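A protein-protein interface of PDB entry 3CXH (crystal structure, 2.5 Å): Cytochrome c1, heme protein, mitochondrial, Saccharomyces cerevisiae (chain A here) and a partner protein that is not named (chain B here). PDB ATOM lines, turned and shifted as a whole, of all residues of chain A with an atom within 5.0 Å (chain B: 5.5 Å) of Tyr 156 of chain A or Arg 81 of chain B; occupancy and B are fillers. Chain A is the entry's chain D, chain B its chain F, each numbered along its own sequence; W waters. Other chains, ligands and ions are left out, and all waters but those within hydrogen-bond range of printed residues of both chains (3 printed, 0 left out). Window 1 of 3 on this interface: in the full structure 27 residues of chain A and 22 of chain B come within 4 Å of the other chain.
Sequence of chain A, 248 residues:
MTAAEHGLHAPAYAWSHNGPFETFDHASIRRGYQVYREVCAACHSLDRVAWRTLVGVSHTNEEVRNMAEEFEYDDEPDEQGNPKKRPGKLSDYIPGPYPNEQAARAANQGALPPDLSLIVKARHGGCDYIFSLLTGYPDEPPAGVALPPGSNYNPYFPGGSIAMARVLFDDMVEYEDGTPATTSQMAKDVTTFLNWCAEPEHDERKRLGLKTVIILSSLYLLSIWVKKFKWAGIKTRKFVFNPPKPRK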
ATOM      1  N   GLY A   7      -9.745   5.659 -26.520  1.00  0.00           N
ATOM      2  CA  GLY A   7     -10.818   5.172 -25.674  1.00  0.00           C
ATOM      3  C   GLY A   7     -10.539   5.703 -24.278  1.00  0.00           C
ATOM      4  O   GLY A   7      -9.391   5.987 -23.937  1.00  0.00           O
ATOM      5  N   LEU A   8     -11.577   5.856 -23.469  1.00  0.00           N
ATOM      6  CA  LEU A   8     -11.406   6.378 -22.121  1.00  0.00           C
ATOM      7  C   LEU A   8     -10.727   5.326 -21.259  1.00  0.00           C
ATOM      8  O   LEU A   8     -11.056   4.137 -21.331  1.00  0.00           O
ATOM      9  CB  LEU A   8     -12.770   6.795 -21.542  1.00  0.00           C
ATOM     10  CG  LEU A   8     -12.875   7.837 -20.417  1.00  0.00           C
ATOM     11  CD1 LEU A   8     -12.740   7.200 -19.065  1.00  0.00           C
ATOM     12  CD2 LEU A   8     -11.840   8.933 -20.599  1.00  0.00           C
ATOM     13  N   HIS A   9      -9.738   5.767 -20.488  1.00  0.00           N
ATOM     14  CA  HIS A   9      -8.996   4.879 -19.603  1.00  0.00           C
ATOM     15  C   HIS A   9      -9.927   4.322 -18.533  1.00  0.00           C
ATOM     16  O   HIS A   9     -10.619   5.081 -17.849  1.00  0.00           O
ATOM     17  CB  HIS A   9      -7.845   5.641 -18.943  1.00  0.00           C
ATOM     18  CG  HIS A   9      -7.019   4.807 -18.008  1.00  0.00           C
ATOM     19  ND1 HIS A   9      -7.354   4.619 -16.680  1.00  0.00           N
ATOM     20  CD2 HIS A   9      -5.865   4.121 -18.205  1.00  0.00           C
ATOM     21  CE1 HIS A   9      -6.442   3.854 -16.103  1.00  0.00           C
ATOM     22  NE2 HIS A   9      -5.529   3.539 -17.005  1.00  0.00           N
ATOM     23  N   ALA A  10      -9.962   3.000 -18.412  1.00  0.00           N
ATOM     24  CA  ALA A  10     -10.788   2.338 -17.414  1.00  0.00           C
ATOM     25  C   ALA A  10     -10.133   2.485 -16.038  1.00  0.00           C
ATOM     26  O   ALA A  10      -8.967   2.146 -15.863  1.00  0.00           O
ATOM     27  CB  ALA A  10     -10.958   0.880 -17.769  1.00  0.00           C
ATOM     28  N   PRO A  11     -10.867   3.042 -15.056  1.00  0.00           N
ATOM     29  CA  PRO A  11     -10.385   3.259 -13.688  1.00  0.00           C
ATOM     30  C   PRO A  11     -10.240   1.995 -12.849  1.00  0.00           C
ATOM     31  O   PRO A  11     -10.854   0.965 -13.128  1.00  0.00           O
ATOM     32  CB  PRO A  11     -11.431   4.210 -13.114  1.00  0.00           C
ATOM     33  CG  PRO A  11     -12.668   3.771 -13.784  1.00  0.00           C
ATOM     34  CD  PRO A  11     -12.216   3.617 -15.217  1.00  0.00           C
ATOM     35  N   TYR A  13     -11.104  -0.213 -10.024  1.00  0.00           N
ATOM     36  CA  TYR A  13     -12.071  -0.629  -9.015  1.00  0.00           C
ATOM     37  C   TYR A  13     -11.401  -1.599  -8.051  1.00  0.00           C
ATOM     38  O   TYR A  13     -10.407  -2.242  -8.395  1.00  0.00           O
ATOM     39  CB  TYR A  13     -13.291  -1.266  -9.674  1.00  0.00           C
ATOM     40  CG  TYR A  13     -14.107  -0.279 -10.471  1.00  0.00           C
ATOM     41  CD1 TYR A  13     -15.069   0.525  -9.851  1.00  0.00           C
ATOM     42  CD2 TYR A  13     -13.902  -0.125 -11.840  1.00  0.00           C
ATOM     43  CE1 TYR A  13     -15.806   1.467 -10.579  1.00  0.00           C
ATOM     44  CE2 TYR A  13     -14.634   0.811 -12.579  1.00  0.00           C
ATOM     45  CZ  TYR A  13     -15.581   1.604 -11.941  1.00  0.00           C
ATOM     46  OH  TYR A  13     -16.296   2.532 -12.665  1.00  0.00           O
ATOM     47  N   TYR A 129     -11.692  -2.899 -17.482  1.00  0.00           N
ATOM     48  CA  TYR A 129     -12.206  -2.553 -18.793  1.00  0.00           C
ATOM     49  C   TYR A 129     -13.594  -3.124 -19.017  1.00  0.00           C
ATOM     50  O   TYR A 129     -14.488  -2.400 -19.442  1.00  0.00           O
ATOM     51  CB  TYR A 129     -11.265  -3.020 -19.907  1.00  0.00           C
ATOM     52  CG  TYR A 129     -11.884  -2.885 -21.274  1.00  0.00           C
ATOM     53  CD1 TYR A 129     -12.085  -1.627 -21.845  1.00  0.00           C
ATOM     54  CD2 TYR A 129     -12.355  -4.007 -21.961  1.00  0.00           C
ATOM     55  CE1 TYR A 129     -12.745  -1.486 -23.052  1.00  0.00           C
ATOM     56  CE2 TYR A 129     -13.017  -3.882 -23.172  1.00  0.00           C
ATOM     57  CZ  TYR A 129     -13.215  -2.618 -23.711  1.00  0.00           C
ATOM     58  OH  TYR A 129     -13.920  -2.477 -24.887  1.00  0.00           O
ATOM     59  N   SER A 132     -16.212  -1.398 -16.873  1.00  0.00           N
ATOM     60  CA  SER A 132     -16.378  -0.029 -17.346  1.00  0.00           C
ATOM     61  C   SER A 132     -17.137   0.049 -18.665  1.00  0.00           C
ATOM     62  O   SER A 132     -17.808   1.036 -18.934  1.00  0.00           O
ATOM     63  CB  SER A 132     -15.024   0.657 -17.507  1.00  0.00           C
ATOM     64  OG  SER A 132     -14.372   0.827 -16.261  1.00  0.00           O
ATOM     65  N   LEU A 133     -17.004  -0.974 -19.503  1.00  0.00           N
ATOM     66  CA  LEU A 133     -17.694  -0.993 -20.784  1.00  0.00           C
ATOM     67  C   LEU A 133     -19.173  -1.293 -20.556  1.00  0.00           C
ATOM     68  O   LEU A 133     -20.046  -0.643 -21.128  1.00  0.00           O
ATOM     69  CB  LEU A 133     -17.088  -2.057 -21.699  1.00  0.00           C
ATOM     70  CG  LEU A 133     -17.620  -2.104 -23.136  1.00  0.00           C
ATOM     71  CD1 LEU A 133     -17.037  -0.947 -23.937  1.00  0.00           C
ATOM     72  CD2 LEU A 133     -17.238  -3.421 -23.782  1.00  0.00           C
ATOM     73  N   THR A 135     -20.976  -0.746 -17.865  1.00  0.00           N
ATOM     74  CA  THR A 135     -21.682   0.242 -17.061  1.00  0.00           C
ATOM     75  C   THR A 135     -21.441   1.663 -17.553  1.00  0.00           C
ATOM     76  O   THR A 135     -21.998   2.621 -16.998  1.00  0.00           O
ATOM     77  CB  THR A 135     -21.241   0.167 -15.586  1.00  0.00           C
ATOM     78  OG1 THR A 135     -19.831   0.384 -15.497  1.00  0.00           O
ATOM     79  CG2 THR A 135     -21.575  -1.188 -14.987  1.00  0.00           C
ATOM     80  N   GLY A 136     -20.655   1.791 -18.621  1.00  0.00           N
ATOM     81  CA  GLY A 136     -20.326   3.106 -19.141  1.00  0.00           C
ATOM     82  C   GLY A 136     -21.062   3.592 -20.368  1.00  0.00           C
ATOM     83  O   GLY A 136     -20.534   4.429 -21.099  1.00  0.00           O
ATOM     84  N   ASN A 154     -20.013   4.413 -26.498  1.00  0.00           N
ATOM     85  CA  ASN A 154     -19.423   3.972 -25.245  1.00  0.00           C
ATOM     86  C   ASN A 154     -18.005   4.510 -25.298  1.00  0.00           C
ATOM     87  O   ASN A 154     -17.196   4.065 -26.106  1.00  0.00           O
ATOM     88  CB  ASN A 154     -19.415   2.456 -25.103  1.00  0.00           C
ATOM     89  CG  ASN A 154     -18.991   2.014 -23.717  1.00  0.00           C
ATOM     90  OD1 ASN A 154     -17.956   2.454 -23.198  1.00  0.00           O
ATOM     91  ND2 ASN A 154     -19.788   1.150 -23.101  1.00  0.00           N
ATOM     92  N   PRO A 155     -17.670   5.438 -24.395  1.00  0.00           N
ATOM     93  CA  PRO A 155     -16.346   6.063 -24.330  1.00  0.00           C
ATOM     94  C   PRO A 155     -15.151   5.149 -24.051  1.00  0.00           C
ATOM     95  O   PRO A 155     -14.043   5.454 -24.467  1.00  0.00           O
ATOM     96  CB  PRO A 155     -16.534   7.110 -23.237  1.00  0.00           C
ATOM     97  CG  PRO A 155     -17.445   6.396 -22.287  1.00  0.00           C
ATOM     98  CD  PRO A 155     -18.483   5.821 -23.226  1.00  0.00           C
ATOM     99  N   TYR A 156     -15.363   4.043 -23.349  1.00  0.00           N
ATOM    100  CA  TYR A 156     -14.264   3.129 -23.039  1.00  0.00           C
ATOM    101  C   TYR A 156     -13.838   2.278 -24.237  1.00  0.00           C
ATOM    102  O   TYR A 156     -12.735   1.730 -24.262  1.00  0.00           O
ATOM    103  CB  TYR A 156     -14.635   2.234 -21.861  1.00  0.00           C
ATOM    104  CG  TYR A 156     -14.974   3.009 -20.612  1.00  0.00           C
ATOM    105  CD1 TYR A 156     -16.299   3.296 -20.288  1.00  0.00           C
ATOM    106  CD2 TYR A 156     -13.969   3.480 -19.767  1.00  0.00           C
ATOM    107  CE1 TYR A 156     -16.616   4.036 -19.151  1.00  0.00           C
ATOM    108  CE2 TYR A 156     -14.272   4.219 -18.631  1.00  0.00           C
ATOM    109  CZ  TYR A 156     -15.600   4.496 -18.329  1.00  0.00           C
ATOM    110  OH  TYR A 156     -15.908   5.246 -17.221  1.00  0.00           O
ATOM    111  N   PHE A 157     -14.717   2.172 -25.224  1.00  0.00           N
ATOM    112  CA  PHE A 157     -14.432   1.406 -26.426  1.00  0.00           C
ATOM    113  C   PHE A 157     -13.623   2.264 -27.399  1.00  0.00           C
ATOM    114  O   PHE A 157     -13.968   3.416 -27.647  1.00  0.00           O
ATOM    115  CB  PHE A 157     -15.742   0.962 -27.077  1.00  0.00           C
ATOM    116  CG  PHE A 157     -15.558  -0.020 -28.195  1.00  0.00           C
ATOM    117  CD1 PHE A 157     -15.179  -1.336 -27.923  1.00  0.00           C
ATOM    118  CD2 PHE A 157     -15.757   0.366 -29.523  1.00  0.00           C
ATOM    119  CE1 PHE A 157     -15.003  -2.256 -28.957  1.00  0.00           C
ATOM    120  CE2 PHE A 157     -15.584  -0.548 -30.569  1.00  0.00           C
ATOM    121  CZ  PHE A 157     -15.205  -1.862 -30.284  1.00  0.00           C
ATOM    122  N   PRO A 158     -12.506   1.728 -27.931  1.00  0.00           N
ATOM    123  CA  PRO A 158     -11.706   2.526 -28.872  1.00  0.00           C
ATOM    124  C   PRO A 158     -12.554   2.971 -30.065  1.00  0.00           C
ATOM    125  O   PRO A 158     -13.259   2.165 -30.665  1.00  0.00           O
ATOM    126  CB  PRO A 158     -10.590   1.558 -29.272  1.00  0.00           C
ATOM    127  CG  PRO A 158     -10.388   0.749 -28.008  1.00  0.00           C
ATOM    128  CD  PRO A 158     -11.827   0.457 -27.608  1.00  0.00           C
ATOM    129  N   GLN B  76     -26.048   1.819  -7.526  1.00  0.00           N
ATOM    130  CA  GLN B  76     -25.051   2.469  -6.688  1.00  0.00           C
ATOM    131  C   GLN B  76     -24.061   3.348  -7.448  1.00  0.00           C
ATOM    132  O   GLN B  76     -23.675   4.420  -6.970  1.00  0.00           O
ATOM    133  CB  GLN B  76     -24.300   1.427  -5.870  1.00  0.00           C
ATOM    134  CG  GLN B  76     -25.185   0.577  -4.978  1.00  0.00           C
ATOM    135  CD  GLN B  76     -25.688  -0.686  -5.651  1.00  0.00           C
ATOM    136  OE1 GLN B  76     -25.931  -1.696  -4.988  1.00  0.00           O
ATOM    137  NE2 GLN B  76     -25.844  -0.639  -6.970  1.00  0.00           N
ATOM    138  N   LEU B  77     -23.644   2.900  -8.628  1.00  0.00           N
ATOM    139  CA  LEU B  77     -22.702   3.678  -9.421  1.00  0.00           C
ATOM    140  C   LEU B  77     -23.360   4.963  -9.922  1.00  0.00           C
ATOM    141  O   LEU B  77     -22.761   6.040  -9.856  1.00  0.00           O
ATOM    142  CB  LEU B  77     -22.155   2.855 -10.589  1.00  0.00           C
ATOM    143  CG  LEU B  77     -21.023   3.505 -11.389  1.00  0.00           C
ATOM    144  CD1 LEU B  77     -19.845   3.816 -10.486  1.00  0.00           C
ATOM    145  CD2 LEU B  77     -20.611   2.591 -12.511  1.00  0.00           C
ATOM    146  N   GLU B  78     -24.603   4.855 -10.385  1.00  0.00           N
ATOM    147  CA  GLU B  78     -25.328   6.024 -10.875  1.00  0.00           C
ATOM    148  C   GLU B  78     -25.456   7.079  -9.779  1.00  0.00           C
ATOM    149  O   GLU B  78     -25.311   8.269 -10.045  1.00  0.00           O
ATOM    150  CB  GLU B  78     -26.698   5.626 -11.440  1.00  0.00           C
ATOM    151  CG  GLU B  78     -26.616   5.103 -12.877  1.00  0.00           C
ATOM    152  CD  GLU B  78     -27.886   4.399 -13.353  1.00  0.00           C
ATOM    153  OE1 GLU B  78     -27.770   3.262 -13.877  1.00  0.00           O
ATOM    154  OE2 GLU B  78     -28.992   4.979 -13.217  1.00  0.00           O
ATOM    155  N   ASP B  79     -25.647   6.632  -8.540  1.00  0.00           N
ATOM    156  CA  ASP B  79     -25.755   7.546  -7.408  1.00  0.00           C
ATOM    157  C   ASP B  79     -24.437   8.283  -7.202  1.00  0.00           C
ATOM    158  O   ASP B  79     -24.403   9.515  -7.177  1.00  0.00           O
ATOM    159  CB  ASP B  79     -26.131   6.794  -6.126  1.00  0.00           C
ATOM    160  CG  ASP B  79     -27.518   6.165  -6.194  1.00  0.00           C
ATOM    161  OD1 ASP B  79     -28.288   6.470  -7.140  1.00  0.00           O
ATOM    162  OD2 ASP B  79     -27.837   5.357  -5.291  1.00  0.00           O
ATOM    163  N   LEU B  80     -23.351   7.523  -7.084  1.00  0.00           N
ATOM    164  CA  LEU B  80     -22.029   8.098  -6.886  1.00  0.00           C
ATOM    165  C   LEU B  80     -21.659   9.118  -7.963  1.00  0.00           C
ATOM    166  O   LEU B  80     -21.116  10.181  -7.658  1.00  0.00           O
ATOM    167  CB  LEU B  80     -20.978   6.989  -6.807  1.00  0.00           C
ATOM    168  CG  LEU B  80     -20.923   6.234  -5.479  1.00  0.00           C
ATOM    169  CD1 LEU B  80     -20.030   5.027  -5.593  1.00  0.00           C
ATOM    170  CD2 LEU B  80     -20.415   7.156  -4.393  1.00  0.00           C
ATOM    171  N   ARG B  81     -21.982   8.810  -9.217  1.00  0.00           N
ATOM    172  CA  ARG B  81     -21.681   9.724 -10.315  1.00  0.00           C
ATOM    173  C   ARG B  81     -22.471  11.014 -10.171  1.00  0.00           C
ATOM    174  O   ARG B  81     -21.953  12.104 -10.430  1.00  0.00           O
ATOM    175  CB  ARG B  81     -22.000   9.082 -11.665  1.00  0.00           C
ATOM    176  CG  ARG B  81     -20.913   8.170 -12.200  1.00  0.00           C
ATOM    177  CD  ARG B  81     -21.317   7.577 -13.537  1.00  0.00           C
ATOM    178  NE  ARG B  81     -20.241   6.794 -14.135  1.00  0.00           N
ATOM    179  CZ  ARG B  81     -20.419   5.666 -14.817  1.00  0.00           C
ATOM    180  NH1 ARG B  81     -19.370   5.032 -15.327  1.00  0.00           N
ATOM    181  NH2 ARG B  81     -21.641   5.167 -14.981  1.00  0.00           N
ATOM    182  N   GLU B  82     -23.730  10.875  -9.759  1.00  0.00           N
ATOM    183  CA  GLU B  82     -24.619  12.014  -9.572  1.00  0.00           C
ATOM    184  C   GLU B  82     -24.090  12.887  -8.440  1.00  0.00           C
ATOM    185  O   GLU B  82     -24.068  14.113  -8.551  1.00  0.00           O
ATOM    186  CB  GLU B  82     -26.043  11.537  -9.272  1.00  0.00           C
ATOM    187  CG  GLU B  82     -27.122  12.567  -9.586  1.00  0.00           C
ATOM    188  CD  GLU B  82     -27.038  13.098 -11.014  1.00  0.00           C
ATOM    189  OE1 GLU B  82     -26.794  12.294 -11.948  1.00  0.00           O
ATOM    190  OE2 GLU B  82     -27.205  14.326 -11.200  1.00  0.00           O
ATOM    191  N   HIS B  83     -23.623  12.248  -7.372  1.00  0.00           N
ATOM    192  CA  HIS B  83     -23.068  12.974  -6.244  1.00  0.00           C
ATOM    193  C   HIS B  83     -21.884  13.818  -6.705  1.00  0.00           C
ATOM    194  O   HIS B  83     -21.851  15.025  -6.476  1.00  0.00           O
ATOM    195  CB  HIS B  83     -22.624  12.001  -5.149  1.00  0.00           C
ATOM    196  CG  HIS B  83     -21.815  12.641  -4.064  1.00  0.00           C
ATOM    197  ND1 HIS B  83     -22.384  13.361  -3.035  1.00  0.00           N
ATOM    198  CD2 HIS B  83     -20.477  12.678  -3.855  1.00  0.00           C
ATOM    199  CE1 HIS B  83     -21.431  13.814  -2.239  1.00  0.00           C
ATOM    200  NE2 HIS B  83     -20.264  13.415  -2.714  1.00  0.00           N
ATOM    201  N   PHE B  84     -20.938  13.191  -7.398  1.00  0.00           N
ATOM    202  CA  PHE B  84     -19.758  13.908  -7.865  1.00  0.00           C
ATOM    203  C   PHE B  84     -19.940  14.889  -9.003  1.00  0.00           C
ATOM    204  O   PHE B  84     -19.065  15.715  -9.252  1.00  0.00           O
ATOM    205  CB  PHE B  84     -18.603  12.951  -8.123  1.00  0.00           C
ATOM    206  CG  PHE B  84     -18.003  12.417  -6.863  1.00  0.00           C
ATOM    207  CD1 PHE B  84     -18.459  11.214  -6.312  1.00  0.00           C
ATOM    208  CD2 PHE B  84     -17.030  13.149  -6.182  1.00  0.00           C
ATOM    209  CE1 PHE B  84     -17.959  10.753  -5.104  1.00  0.00           C
ATOM    210  CE2 PHE B  84     -16.519  12.698  -4.969  1.00  0.00           C
ATOM    211  CZ  PHE B  84     -16.986  11.498  -4.428  1.00  0.00           C
ATOM    212  N   LYS B  85     -21.068  14.808  -9.695  1.00  0.00           N
ATOM    213  CA  LYS B  85     -21.350  15.754 -10.771  1.00  0.00           C
ATOM    214  C   LYS B  85     -21.678  17.090 -10.110  1.00  0.00           C
ATOM    215  O   LYS B  85     -21.642  18.138 -10.759  1.00  0.00           O
ATOM    216  CB  LYS B  85     -22.568  15.308 -11.580  1.00  0.00           C
ATOM    217  CG  LYS B  85     -22.276  14.449 -12.792  1.00  0.00           C
ATOM    218  CD  LYS B  85     -23.571  13.835 -13.318  1.00  0.00           C
ATOM    219  CE  LYS B  85     -23.392  13.220 -14.692  1.00  0.00           C
ATOM    220  NZ  LYS B  85     -22.985  14.250 -15.687  1.00  0.00           N
ATOM    221  N   ASN B  86     -21.983  17.033  -8.810  1.00  0.00           N
ATOM    222  CA  ASN B  86     -22.359  18.204  -8.028  1.00  0.00           C
ATOM    223  C   ASN B  86     -21.284  18.888  -7.190  1.00  0.00           C
ATOM    224  O   ASN B  86     -21.565  19.850  -6.471  1.00  0.00           O
ATOM    225  CB  ASN B  86     -23.605  17.896  -7.203  1.00  0.00           C
ATOM    226  CG  ASN B  86     -24.838  17.734  -8.078  1.00  0.00           C
ATOM    227  OD1 ASN B  86     -25.185  18.637  -8.849  1.00  0.00           O
ATOM    228  ND2 ASN B  86     -25.483  16.574  -7.995  1.00  0.00           N
ATOM    229  N   GLN B 130     -15.884  12.604 -17.518  1.00  0.00           N
ATOM    230  CA  GLN B 130     -15.998  11.194 -17.162  1.00  0.00           C
ATOM    231  C   GLN B 130     -14.764  10.720 -16.398  1.00  0.00           C
ATOM    232  O   GLN B 130     -14.876   9.927 -15.467  1.00  0.00           O
ATOM    233  CB  GLN B 130     -16.238  10.339 -18.408  1.00  0.00           C
ATOM    234  CG  GLN B 130     -16.544   8.877 -18.114  1.00  0.00           C
ATOM    235  CD  GLN B 130     -17.833   8.665 -17.328  1.00  0.00           C
ATOM    236  OE1 GLN B 130     -18.567   9.613 -17.034  1.00  0.00           O
ATOM    237  NE2 GLN B 130     -18.118   7.410 -16.995  1.00  0.00           N
ATOM    238  N   LEU B 133     -15.111  11.846 -12.713  1.00  0.00           N
ATOM    239  CA  LEU B 133     -16.074  11.007 -12.008  1.00  0.00           C
ATOM    240  C   LEU B 133     -15.492   9.619 -11.693  1.00  0.00           C
ATOM    241  O   LEU B 133     -15.669   9.098 -10.583  1.00  0.00           O
ATOM    242  CB  LEU B 133     -17.357  10.868 -12.831  1.00  0.00           C
ATOM    243  CG  LEU B 133     -18.078  12.156 -13.250  1.00  0.00           C
ATOM    244  CD1 LEU B 133     -19.286  11.814 -14.102  1.00  0.00           C
ATOM    245  CD2 LEU B 133     -18.504  12.956 -12.027  1.00  0.00           C
ATOM    246  N   ASP B 134     -14.791   9.033 -12.668  1.00  0.00           N
ATOM    247  CA  ASP B 134     -14.168   7.713 -12.502  1.00  0.00           C
ATOM    248  C   ASP B 134     -13.159   7.713 -11.358  1.00  0.00           C
ATOM    249  O   ASP B 134     -13.177   6.835 -10.498  1.00  0.00           O
ATOM    250  CB  ASP B 134     -13.444   7.289 -13.784  1.00  0.00           C
ATOM    251  CG  ASP B 134     -14.376   6.719 -14.837  1.00  0.00           C
ATOM    252  OD1 ASP B 134     -15.423   6.121 -14.485  1.00  0.00           O
ATOM    253  OD2 ASP B 134     -14.029   6.853 -16.030  1.00  0.00           O
ATOM    254  N   THR B 137     -15.318   7.811  -8.189  1.00  0.00           N
ATOM    255  CA  THR B 137     -16.198   6.667  -7.968  1.00  0.00           C
ATOM    256  C   THR B 137     -15.523   5.307  -7.882  1.00  0.00           C
ATOM    257  O   THR B 137     -15.971   4.447  -7.126  1.00  0.00           O
ATOM    258  CB  THR B 137     -17.294   6.605  -9.045  1.00  0.00           C
ATOM    259  OG1 THR B 137     -16.689   6.599 -10.345  1.00  0.00           O
ATOM    260  CG2 THR B 137     -18.214   7.812  -8.929  1.00  0.00           C
HETATM  261  O   HOH W   1     -15.876   3.160 -15.336  1.00  0.00           O
HETATM  262  O   HOH W   2     -18.505   2.492 -16.277  1.00  0.00           O
HETATM  263  O   HOH W   3     -11.138   7.309 -16.323  1.00  0.00           O
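O of Thr 135 of chain A sits at hydrogen-bond distance from NH2 of Arg 81 of chain B. The side-chain hydroxyl of Tyr 156 of chain A lies within hydrogen-bond range of the side-chain amide nitrogen of Gln 130 of chain B, 3.1 Å away. The side-chain hydroxyl (OH) of Tyr 156 of chain A lies within hydrogen-bond range of the side-chain carboxylate (OD2) of Asp 134 of chain B.
The backbone NH of Leu 8 of chain A lies within hydrogen-bond range of the backbone carbonyl oxygen of Pro 155 of chain A (2.7 Å). N of Tyr 156 of chain A lies within hydrogen-bond range of OD1 of Asn 154 of chain A, at 3.0 Å. NH1 of Arg 81 of chain B sits close to NE2 of Gln 130 of chain B (3.2 Å).
Leu 8 of chain A touches Asp 134 of chain B (CD1 to OD2, 3.3 Å). CG of Asp 134 of chain B touches CG of Pro 11 of chain A (3.6 Å). OG1 of Thr 135 of chain A touches CD2 of Leu 77 of chain B, 3.8 Å away. Tyr 156 of chain A touches Arg 81 of chain B (OH to NH1, 3.95 Å).
Of the printed residues of chain B, Pro 11 of chain A touches Asp 134. Tyr 156 of chain A touches just these residues of chain B: Arg 81 (3.95 Å), Gln 130 (3.1 Å) and Asp 134 (2.7 Å). Phe 157 of chain A touches none of the printed residues of chain B. Of the printed residues of chain A, Leu 77 of chain B touches Thr 135 (3.8 Å). Arg 81 of chain B touches just these residues of chain A: Thr 135 (3.3 Å) and Tyr 156 (3.95 Å). Asn 86 of chain B touches none of the printed residues of chain A. Printed residues of chain A within 4 Å of Gln 130 of chain B: Tyr 156. Of the printed residues of chain A, Asp 134 of chain B touches Leu 8 (3.3 Å), Pro 11 (3.6 Å) and Tyr 156 (2.7 Å). The nearest printed residue of chain B that does not touch Pro 11 of chain A is Thr 137 of chain B (6.0 Å).
Printed residues of chain A that touch a printed residue of chain B: Leu 8, Pro 11, Thr 135 and Tyr 156. Hydrophobic or aromatic side chains of chain A within 4 Å of the printed part of chain B: Leu 8, Pro 11 and Tyr 156. Along chain A the printed residues that touch a printed residue of chain B span positions 8 to 156. Among the printed residues, no Asp or Glu carboxylate lies within 4 Å of a Lys or Arg side-chain nitrogen of the other chain.
Water W2 lies within hydrogen-bond range of OG1 of Thr 135 of chain A (2.6 Å), NH1 of Arg 81 of chain B (2.8 Å), O of Ser 132 of chain A (3.1 Å) and N of Gly 136 of chain A (3.3 Å). Water W3 bridges O of His 9 of chain A and OD2 of Asp 134 of chain B. Water W1 lies within hydrogen-bond range of OH of Tyr 13 of chain A (2.8 Å), OH of Tyr 156 of chain A (2.8 Å), OG of Ser 132 of chain A (2.9 Å) and OD1 of Asp 134 of chain B (3.1 Å).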
